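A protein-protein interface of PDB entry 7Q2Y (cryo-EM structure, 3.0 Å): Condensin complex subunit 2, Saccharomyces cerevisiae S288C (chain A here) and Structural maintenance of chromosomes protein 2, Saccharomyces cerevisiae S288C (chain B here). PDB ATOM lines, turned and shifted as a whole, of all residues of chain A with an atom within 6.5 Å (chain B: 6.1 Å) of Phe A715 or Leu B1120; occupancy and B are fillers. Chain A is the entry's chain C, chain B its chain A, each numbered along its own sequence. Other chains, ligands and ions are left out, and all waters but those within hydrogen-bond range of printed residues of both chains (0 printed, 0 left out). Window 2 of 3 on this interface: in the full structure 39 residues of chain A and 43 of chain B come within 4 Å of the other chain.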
ATOM      1  N   LYS A 643      18.904  -0.551   9.174  1.00  0.00           N
ATOM      2  CA  LYS A 643      19.618   0.159   8.121  1.00  0.00           C
ATOM      3  C   LYS A 643      19.003  -0.177   6.770  1.00  0.00           C
ATOM      4  O   LYS A 643      18.748  -1.348   6.472  1.00  0.00           O
ATOM      5  CB  LYS A 643      21.106  -0.203   8.129  1.00  0.00           C
ATOM      6  CG  LYS A 643      21.768  -0.078   9.493  1.00  0.00           C
ATOM      7  CD  LYS A 643      23.251   0.237   9.369  1.00  0.00           C
ATOM      8  CE  LYS A 643      23.924  -0.651   8.333  1.00  0.00           C
ATOM      9  NZ  LYS A 643      25.392  -0.412   8.271  1.00  0.00           N
ATOM     10  N   VAL A 645      19.723  -0.028   2.773  1.00  0.00           N
ATOM     11  CA  VAL A 645      20.943  -0.003   1.974  1.00  0.00           C
ATOM     12  C   VAL A 645      20.621   0.020   0.483  1.00  0.00           C
ATOM     13  O   VAL A 645      21.389   0.570  -0.315  1.00  0.00           O
ATOM     14  CB  VAL A 645      21.840  -1.203   2.335  1.00  0.00           C
ATOM     15  CG1 VAL A 645      23.109  -1.214   1.496  1.00  0.00           C
ATOM     16  CG2 VAL A 645      22.179  -1.167   3.816  1.00  0.00           C
ATOM     17  N   ASP A 646      19.474  -0.549   0.101  1.00  0.00           N
ATOM     18  CA  ASP A 646      19.061  -0.638  -1.302  1.00  0.00           C
ATOM     19  C   ASP A 646      20.122  -1.379  -2.124  1.00  0.00           C
ATOM     20  O   ASP A 646      20.803  -0.814  -2.984  1.00  0.00           O
ATOM     21  CB  ASP A 646      18.766   0.752  -1.881  1.00  0.00           C
ATOM     22  CG  ASP A 646      17.857   0.699  -3.094  1.00  0.00           C
ATOM     23  OD1 ASP A 646      18.096  -0.141  -3.988  1.00  0.00           O
ATOM     24  OD2 ASP A 646      16.901   1.500  -3.156  1.00  0.00           O
ATOM     25  N   VAL A 647      20.248  -2.672  -1.809  1.00  0.00           N
ATOM     26  CA  VAL A 647      21.354  -3.487  -2.314  1.00  0.00           C
ATOM     27  C   VAL A 647      21.403  -3.473  -3.837  1.00  0.00           C
ATOM     28  O   VAL A 647      22.485  -3.502  -4.436  1.00  0.00           O
ATOM     29  CB  VAL A 647      21.242  -4.923  -1.765  1.00  0.00           C
ATOM     30  CG1 VAL A 647      22.387  -5.786  -2.274  1.00  0.00           C
ATOM     31  CG2 VAL A 647      21.211  -4.909  -0.245  1.00  0.00           C
ATOM     32  N   LEU A 650      23.110  -0.334  -4.882  1.00  0.00           N
ATOM     33  CA  LEU A 650      24.535  -0.444  -4.586  1.00  0.00           C
ATOM     34  C   LEU A 650      25.249  -1.294  -5.629  1.00  0.00           C
ATOM     35  O   LEU A 650      26.343  -0.947  -6.085  1.00  0.00           O
ATOM     36  CB  LEU A 650      24.736  -1.023  -3.185  1.00  0.00           C
ATOM     37  CG  LEU A 650      26.157  -0.968  -2.623  1.00  0.00           C
ATOM     38  CD1 LEU A 650      26.800   0.382  -2.898  1.00  0.00           C
ATOM     39  CD2 LEU A 650      26.157  -1.271  -1.134  1.00  0.00           C
ATOM     40  N   VAL A 654      28.131  -0.031  -8.152  1.00  0.00           N
ATOM     41  CA  VAL A 654      29.442  -0.676  -8.181  1.00  0.00           C
ATOM     42  C   VAL A 654      29.797  -1.092  -9.602  1.00  0.00           C
ATOM     43  O   VAL A 654      30.940  -0.923 -10.048  1.00  0.00           O
ATOM     44  CB  VAL A 654      29.479  -1.869  -7.208  1.00  0.00           C
ATOM     45  CG1 VAL A 654      30.726  -2.704  -7.437  1.00  0.00           C
ATOM     46  CG2 VAL A 654      29.441  -1.376  -5.772  1.00  0.00           C
ATOM     47  N   ASP A 710      25.572   4.667   6.032  1.00  0.00           N
ATOM     48  CA  ASP A 710      25.012   3.321   6.095  1.00  0.00           C
ATOM     49  C   ASP A 710      25.876   2.302   5.362  1.00  0.00           C
ATOM     50  O   ASP A 710      25.970   1.148   5.796  1.00  0.00           O
ATOM     51  CB  ASP A 710      23.594   3.318   5.524  1.00  0.00           C
ATOM     52  CG  ASP A 710      22.545   3.641   6.570  1.00  0.00           C
ATOM     53  OD1 ASP A 710      22.461   2.909   7.577  1.00  0.00           O
ATOM     54  OD2 ASP A 710      21.803   4.629   6.384  1.00  0.00           O
ATOM     55  N   ILE A 711      26.507   2.698   4.254  1.00  0.00           N
ATOM     56  CA  ILE A 711      27.285   1.758   3.455  1.00  0.00           C
ATOM     57  C   ILE A 711      28.536   1.336   4.212  1.00  0.00           C
ATOM     58  O   ILE A 711      29.253   2.167   4.786  1.00  0.00           O
ATOM     59  CB  ILE A 711      27.644   2.375   2.091  1.00  0.00           C
ATOM     60  CG1 ILE A 711      26.380   2.786   1.336  1.00  0.00           C
ATOM     61  CG2 ILE A 711      28.464   1.400   1.261  1.00  0.00           C
ATOM     62  CD1 ILE A 711      25.362   1.679   1.198  1.00  0.00           C
ATOM     63  N   SER A 712      28.805   0.033   4.213  1.00  0.00           N
ATOM     64  CA  SER A 712      29.997  -0.537   4.821  1.00  0.00           C
ATOM     65  C   SER A 712      30.745  -1.354   3.777  1.00  0.00           C
ATOM     66  O   SER A 712      30.232  -1.637   2.692  1.00  0.00           O
ATOM     67  CB  SER A 712      29.648  -1.407   6.037  1.00  0.00           C
ATOM     68  OG  SER A 712      29.062  -0.631   7.068  1.00  0.00           O
ATOM     69  N   THR A 713      31.980  -1.733   4.115  1.00  0.00           N
ATOM     70  CA  THR A 713      32.794  -2.507   3.181  1.00  0.00           C
ATOM     71  C   THR A 713      32.225  -3.904   2.959  1.00  0.00           C
ATOM     72  O   THR A 713      32.444  -4.497   1.897  1.00  0.00           O
ATOM     73  CB  THR A 713      34.239  -2.587   3.679  1.00  0.00           C
ATOM     74  OG1 THR A 713      35.060  -3.202   2.676  1.00  0.00           O
ATOM     75  CG2 THR A 713      34.332  -3.388   4.970  1.00  0.00           C
ATOM     76  N   SER A 714      31.496  -4.441   3.940  1.00  0.00           N
ATOM     77  CA  SER A 714      30.893  -5.760   3.778  1.00  0.00           C
ATOM     78  C   SER A 714      29.836  -5.753   2.681  1.00  0.00           C
ATOM     79  O   SER A 714      29.741  -6.702   1.892  1.00  0.00           O
ATOM     80  CB  SER A 714      30.293  -6.224   5.104  1.00  0.00           C
ATOM     81  OG  SER A 714      29.163  -5.443   5.450  1.00  0.00           O
ATOM     82  N   PHE A 715      29.029  -4.693   2.616  1.00  0.00           N
ATOM     83  CA  PHE A 715      28.022  -4.594   1.564  1.00  0.00           C
ATOM     84  C   PHE A 715      28.667  -4.491   0.188  1.00  0.00           C
ATOM     85  O   PHE A 715      28.188  -5.096  -0.777  1.00  0.00           O
ATOM     86  CB  PHE A 715      27.111  -3.396   1.821  1.00  0.00           C
ATOM     87  CG  PHE A 715      25.825  -3.757   2.494  1.00  0.00           C
ATOM     88  CD1 PHE A 715      24.853  -4.473   1.817  1.00  0.00           C
ATOM     89  CD2 PHE A 715      25.593  -3.397   3.807  1.00  0.00           C
ATOM     90  CE1 PHE A 715      23.669  -4.812   2.436  1.00  0.00           C
ATOM     91  CE2 PHE A 715      24.415  -3.735   4.430  1.00  0.00           C
ATOM     92  CZ  PHE A 715      23.450  -4.444   3.745  1.00  0.00           C
ATOM     93  N   CYS A 716      29.752  -3.722   0.078  1.00  0.00           N
ATOM     94  CA  CYS A 716      30.463  -3.632  -1.191  1.00  0.00           C
ATOM     95  C   CYS A 716      31.061  -4.978  -1.581  1.00  0.00           C
ATOM     96  O   CYS A 716      31.047  -5.355  -2.757  1.00  0.00           O
ATOM     97  CB  CYS A 716      31.546  -2.559  -1.109  1.00  0.00           C
ATOM     98  SG  CYS A 716      30.928  -0.923  -0.649  1.00  0.00           S
ATOM     99  N   PHE A 717      31.588  -5.718  -0.602  1.00  0.00           N
ATOM    100  CA  PHE A 717      32.107  -7.054  -0.882  1.00  0.00           C
ATOM    101  C   PHE A 717      31.003  -7.984  -1.373  1.00  0.00           C
ATOM    102  O   PHE A 717      31.204  -8.753  -2.321  1.00  0.00           O
ATOM    103  CB  PHE A 717      32.775  -7.624   0.370  1.00  0.00           C
ATOM    104  CG  PHE A 717      33.483  -8.928   0.141  1.00  0.00           C
ATOM    105  CD1 PHE A 717      34.275  -9.117  -0.978  1.00  0.00           C
ATOM    106  CD2 PHE A 717      33.358  -9.966   1.049  1.00  0.00           C
ATOM    107  CE1 PHE A 717      34.927 -10.317  -1.188  1.00  0.00           C
ATOM    108  CE2 PHE A 717      34.008 -11.167   0.845  1.00  0.00           C
ATOM    109  CZ  PHE A 717      34.794 -11.342  -0.275  1.00  0.00           C
ATOM    110  N   ILE A 718      29.828  -7.923  -0.743  1.00  0.00           N
ATOM    111  CA  ILE A 718      28.711  -8.769  -1.159  1.00  0.00           C
ATOM    112  C   ILE A 718      28.255  -8.402  -2.567  1.00  0.00           C
ATOM    113  O   ILE A 718      27.955  -9.278  -3.389  1.00  0.00           O
ATOM    114  CB  ILE A 718      27.559  -8.670  -0.142  1.00  0.00           C
ATOM    115  CG1 ILE A 718      27.967  -9.315   1.184  1.00  0.00           C
ATOM    116  CG2 ILE A 718      26.297  -9.322  -0.692  1.00  0.00           C
ATOM    117  CD1 ILE A 718      26.811  -9.563   2.130  1.00  0.00           C
ATOM    118  N   CYS A 719      28.191  -7.103  -2.867  1.00  0.00           N
ATOM    119  CA  CYS A 719      27.802  -6.672  -4.207  1.00  0.00           C
ATOM    120  C   CYS A 719      28.825  -7.110  -5.250  1.00  0.00           C
ATOM    121  O   CYS A 719      28.455  -7.513  -6.359  1.00  0.00           O
ATOM    122  CB  CYS A 719      27.617  -5.156  -4.238  1.00  0.00           C
ATOM    123  SG  CYS A 719      26.184  -4.567  -3.306  1.00  0.00           S
ATOM    124  N   LEU A 720      30.115  -7.035  -4.914  1.00  0.00           N
ATOM    125  CA  LEU A 720      31.145  -7.509  -5.831  1.00  0.00           C
ATOM    126  C   LEU A 720      31.032  -9.011  -6.057  1.00  0.00           C
ATOM    127  O   LEU A 720      31.221  -9.495  -7.179  1.00  0.00           O
ATOM    128  CB  LEU A 720      32.529  -7.146  -5.295  1.00  0.00           C
ATOM    129  CG  LEU A 720      33.708  -7.325  -6.252  1.00  0.00           C
ATOM    130  CD1 LEU A 720      33.804  -6.146  -7.208  1.00  0.00           C
ATOM    131  CD2 LEU A 720      35.004  -7.495  -5.477  1.00  0.00           C
ATOM    132  N   HIS A 722      28.233 -10.733  -5.883  1.00  0.00           N
ATOM    133  CA  HIS A 722      27.067 -10.911  -6.743  1.00  0.00           C
ATOM    134  C   HIS A 722      27.400 -10.595  -8.196  1.00  0.00           C
ATOM    135  O   HIS A 722      26.968 -11.308  -9.111  1.00  0.00           O
ATOM    136  CB  HIS A 722      25.916 -10.031  -6.255  1.00  0.00           C
ATOM    137  CG  HIS A 722      25.064 -10.675  -5.206  1.00  0.00           C
ATOM    138  ND1 HIS A 722      25.246 -10.453  -3.859  1.00  0.00           N
ATOM    139  CD2 HIS A 722      24.022 -11.535  -5.308  1.00  0.00           C
ATOM    140  CE1 HIS A 722      24.354 -11.148  -3.175  1.00  0.00           C
ATOM    141  NE2 HIS A 722      23.600 -11.813  -4.031  1.00  0.00           N
ATOM    142  N   LEU B1118      16.591 -16.486   1.902  1.00  0.00           N
ATOM    143  CA  LEU B1118      16.912 -15.698   0.722  1.00  0.00           C
ATOM    144  C   LEU B1118      17.783 -14.512   1.110  1.00  0.00           C
ATOM    145  O   LEU B1118      17.579 -13.898   2.163  1.00  0.00           O
ATOM    146  CB  LEU B1118      15.640 -15.206   0.025  1.00  0.00           C
ATOM    147  CG  LEU B1118      14.884 -16.228  -0.826  1.00  0.00           C
ATOM    148  CD1 LEU B1118      13.781 -15.549  -1.620  1.00  0.00           C
ATOM    149  CD2 LEU B1118      15.838 -16.967  -1.750  1.00  0.00           C
ATOM    150  N   ASP B1119      18.754 -14.194   0.258  1.00  0.00           N
ATOM    151  CA  ASP B1119      19.632 -13.066   0.520  1.00  0.00           C
ATOM    152  C   ASP B1119      18.900 -11.747   0.266  1.00  0.00           C
ATOM    153  O   ASP B1119      17.752 -11.714  -0.188  1.00  0.00           O
ATOM    154  CB  ASP B1119      20.913 -13.182  -0.315  1.00  0.00           C
ATOM    155  CG  ASP B1119      20.672 -13.085  -1.821  1.00  0.00           C
ATOM    156  OD1 ASP B1119      19.814 -12.302  -2.276  1.00  0.00           O
ATOM    157  OD2 ASP B1119      21.364 -13.813  -2.563  1.00  0.00           O
ATOM    158  N   LEU B1120      19.587 -10.645   0.575  1.00  0.00           N
ATOM    159  CA  LEU B1120      18.973  -9.328   0.446  1.00  0.00           C
ATOM    160  C   LEU B1120      18.616  -9.015  -1.003  1.00  0.00           C
ATOM    161  O   LEU B1120      17.539  -8.475  -1.281  1.00  0.00           O
ATOM    162  CB  LEU B1120      19.908  -8.261   1.015  1.00  0.00           C
ATOM    163  CG  LEU B1120      20.336  -8.476   2.468  1.00  0.00           C
ATOM    164  CD1 LEU B1120      21.494  -7.565   2.831  1.00  0.00           C
ATOM    165  CD2 LEU B1120      19.163  -8.259   3.410  1.00  0.00           C
ATOM    166  N   SER B1121      19.509  -9.343  -1.940  1.00  0.00           N
ATOM    167  CA  SER B1121      19.242  -9.068  -3.347  1.00  0.00           C
ATOM    168  C   SER B1121      18.041  -9.863  -3.847  1.00  0.00           C
ATOM    169  O   SER B1121      17.158  -9.319  -4.522  1.00  0.00           O
ATOM    170  CB  SER B1121      20.482  -9.380  -4.185  1.00  0.00           C
ATOM    171  OG  SER B1121      20.239  -9.151  -5.562  1.00  0.00           O
ATOM    172  N   HIS B1122      17.989 -11.156  -3.520  1.00  0.00           N
ATOM    173  CA  HIS B1122      16.855 -11.978  -3.933  1.00  0.00           C
ATOM    174  C   HIS B1122      15.565 -11.517  -3.266  1.00  0.00           C
ATOM    175  O   HIS B1122      14.503 -11.520  -3.895  1.00  0.00           O
ATOM    176  CB  HIS B1122      17.124 -13.451  -3.623  1.00  0.00           C
ATOM    177  CG  HIS B1122      18.198 -14.059  -4.470  1.00  0.00           C
ATOM    178  ND1 HIS B1122      18.716 -15.313  -4.228  1.00  0.00           N
ATOM    179  CD2 HIS B1122      18.849 -13.587  -5.560  1.00  0.00           C
ATOM    180  CE1 HIS B1122      19.641 -15.587  -5.131  1.00  0.00           C
ATOM    181  NE2 HIS B1122      19.741 -14.556  -5.951  1.00  0.00           N
ATOM    182  N   THR B1123      15.638 -11.124  -1.992  1.00  0.00           N
ATOM    183  CA  THR B1123      14.452 -10.628  -1.299  1.00  0.00           C
ATOM    184  C   THR B1123      13.918  -9.366  -1.965  1.00  0.00           C
ATOM    185  O   THR B1123      12.710  -9.233  -2.200  1.00  0.00           O
ATOM    186  CB  THR B1123      14.787 -10.365   0.171  1.00  0.00           C
ATOM    187  OG1 THR B1123      15.297 -11.563   0.769  1.00  0.00           O
ATOM    188  CG2 THR B1123      13.554  -9.913   0.931  1.00  0.00           C
ATOM    189  N   GLN B1124      14.814  -8.430  -2.290  1.00  0.00           N
ATOM    190  CA  GLN B1124      14.398  -7.203  -2.961  1.00  0.00           C
ATOM    191  C   GLN B1124      13.820  -7.494  -4.339  1.00  0.00           C
ATOM    192  O   GLN B1124      12.810  -6.900  -4.734  1.00  0.00           O
ATOM    193  CB  GLN B1124      15.580  -6.239  -3.067  1.00  0.00           C
ATOM    194  CG  GLN B1124      15.182  -4.782  -3.221  1.00  0.00           C
ATOM    195  CD  GLN B1124      16.378  -3.871  -3.410  1.00  0.00           C
ATOM    196  OE1 GLN B1124      17.509  -4.335  -3.547  1.00  0.00           O
ATOM    197  NE2 GLN B1124      16.132  -2.566  -3.419  1.00  0.00           N
ATOM    198  N   ASN B1125      14.450  -8.404  -5.088  1.00  0.00           N
ATOM    199  CA  ASN B1125      13.941  -8.749  -6.411  1.00  0.00           C
ATOM    200  C   ASN B1125      12.557  -9.381  -6.323  1.00  0.00           C
ATOM    201  O   ASN B1125      11.669  -9.060  -7.121  1.00  0.00           O
ATOM    202  CB  ASN B1125      14.917  -9.690  -7.119  1.00  0.00           C
ATOM    203  CG  ASN B1125      14.517  -9.971  -8.553  1.00  0.00           C
ATOM    204  OD1 ASN B1125      14.167 -11.098  -8.902  1.00  0.00           O
ATOM    205  ND2 ASN B1125      14.567  -8.945  -9.394  1.00  0.00           N
ATOM    206  N   LYS B1145      12.716  -8.429   6.876  1.00  0.00           N
ATOM    207  CA  LYS B1145      13.763  -7.707   6.172  1.00  0.00           C
ATOM    208  C   LYS B1145      13.153  -6.617   5.302  1.00  0.00           C
ATOM    209  O   LYS B1145      12.055  -6.783   4.762  1.00  0.00           O
ATOM    210  CB  LYS B1145      14.603  -8.656   5.312  1.00  0.00           C
ATOM    211  CG  LYS B1145      15.470  -9.609   6.116  1.00  0.00           C
ATOM    212  CD  LYS B1145      16.433 -10.371   5.223  1.00  0.00           C
ATOM    213  CE  LYS B1145      15.715 -11.450   4.433  1.00  0.00           C
ATOM    214  NZ  LYS B1145      16.669 -12.309   3.681  1.00  0.00           N
ATOM    215  N   GLY B1147      13.674  -5.706   2.427  1.00  0.00           N
ATOM    216  CA  GLY B1147      13.635  -5.920   0.989  1.00  0.00           C
ATOM    217  C   GLY B1147      12.239  -5.970   0.399  1.00  0.00           C
ATOM    218  O   GLY B1147      12.005  -5.436  -0.688  1.00  0.00           O
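Val A647 touches Leu B1120 (CG2 to CB, 3.8 Å).
Val A647 touches Gln B1124 (N to OE1, 3.6 Å).
CE1 of Phe A715 touches CD1 of Leu B1120, at 3.5 Å.
Ser B1121 touches His A722.
The side-chain sulfur of Cys A719 is in hydrogen-bond range of the backbone carbonyl oxygen of Phe A715 (3.3 Å).
A ring nitrogen (ND1) of His A722 sits at hydrogen-bond distance from the backbone carbonyl oxygen (O) of Ile A718.
The side-chain carboxylate (OD1) of Asp B1119 is in hydrogen-bond range of the backbone NH (N) of Ser B1121 (3.0 Å).
The side-chain carboxylate (OD1) of Asp B1119 lies within hydrogen-bond range of the backbone NH (N) of His B1122.
The backbone carbonyl oxygen of Asp B1119 lies within hydrogen-bond range of the side-chain hydroxyl of Thr B1123 (2.6 Å).
Of the printed residues of chain B, Asp A646 touches Gln B1124 (3.2 Å).
Of the printed residues of chain B, Phe A715 touches Leu B1120 (3.5 Å).
Printed residues of chain B within 4 Å of His A722: Asp B1119 (3.3 Å) and Ser B1121 (3.96 Å).
Of the printed residues of chain A, Asp B1119 touches His A722 (3.3 Å).
Leu B1120 touches just these residues of chain A: Val A647 and Phe A715.
The nearest residue of chain A that does not touch Leu B1120 is Ile A718 (5.7 Å).
The nearest printed residue of chain B that does not touch Asp A646 is Leu B1120 (7.6 Å).
The side-chain carboxylate of Asp B1119 is in hydrogen-bond range of a ring nitrogen (NE2) of His A722 (3.3 Å).
NE2 of Gln B1124 sits at hydrogen-bond distance from OD1 of Asp A646.
Of the 18 printed residues of chain A, 4 touch a printed residue of chain B.
Hydrophobic or aromatic side chains of chain A that line the printed part of chain B: Val A647, Phe A715 and His A722.
Along chain A the printed residues that touch a printed residue of chain B span positions 646 to 722.
Hydrophobic or aromatic side chains of chain B that line the printed part of chain A: Leu B1120.
Among the printed residues, 6 pairs touch across the chains.
Among the printed residues, no Asp or Glu carboxylate lies within 4 Å of a Lys or Arg side-chain nitrogen of the other chain.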
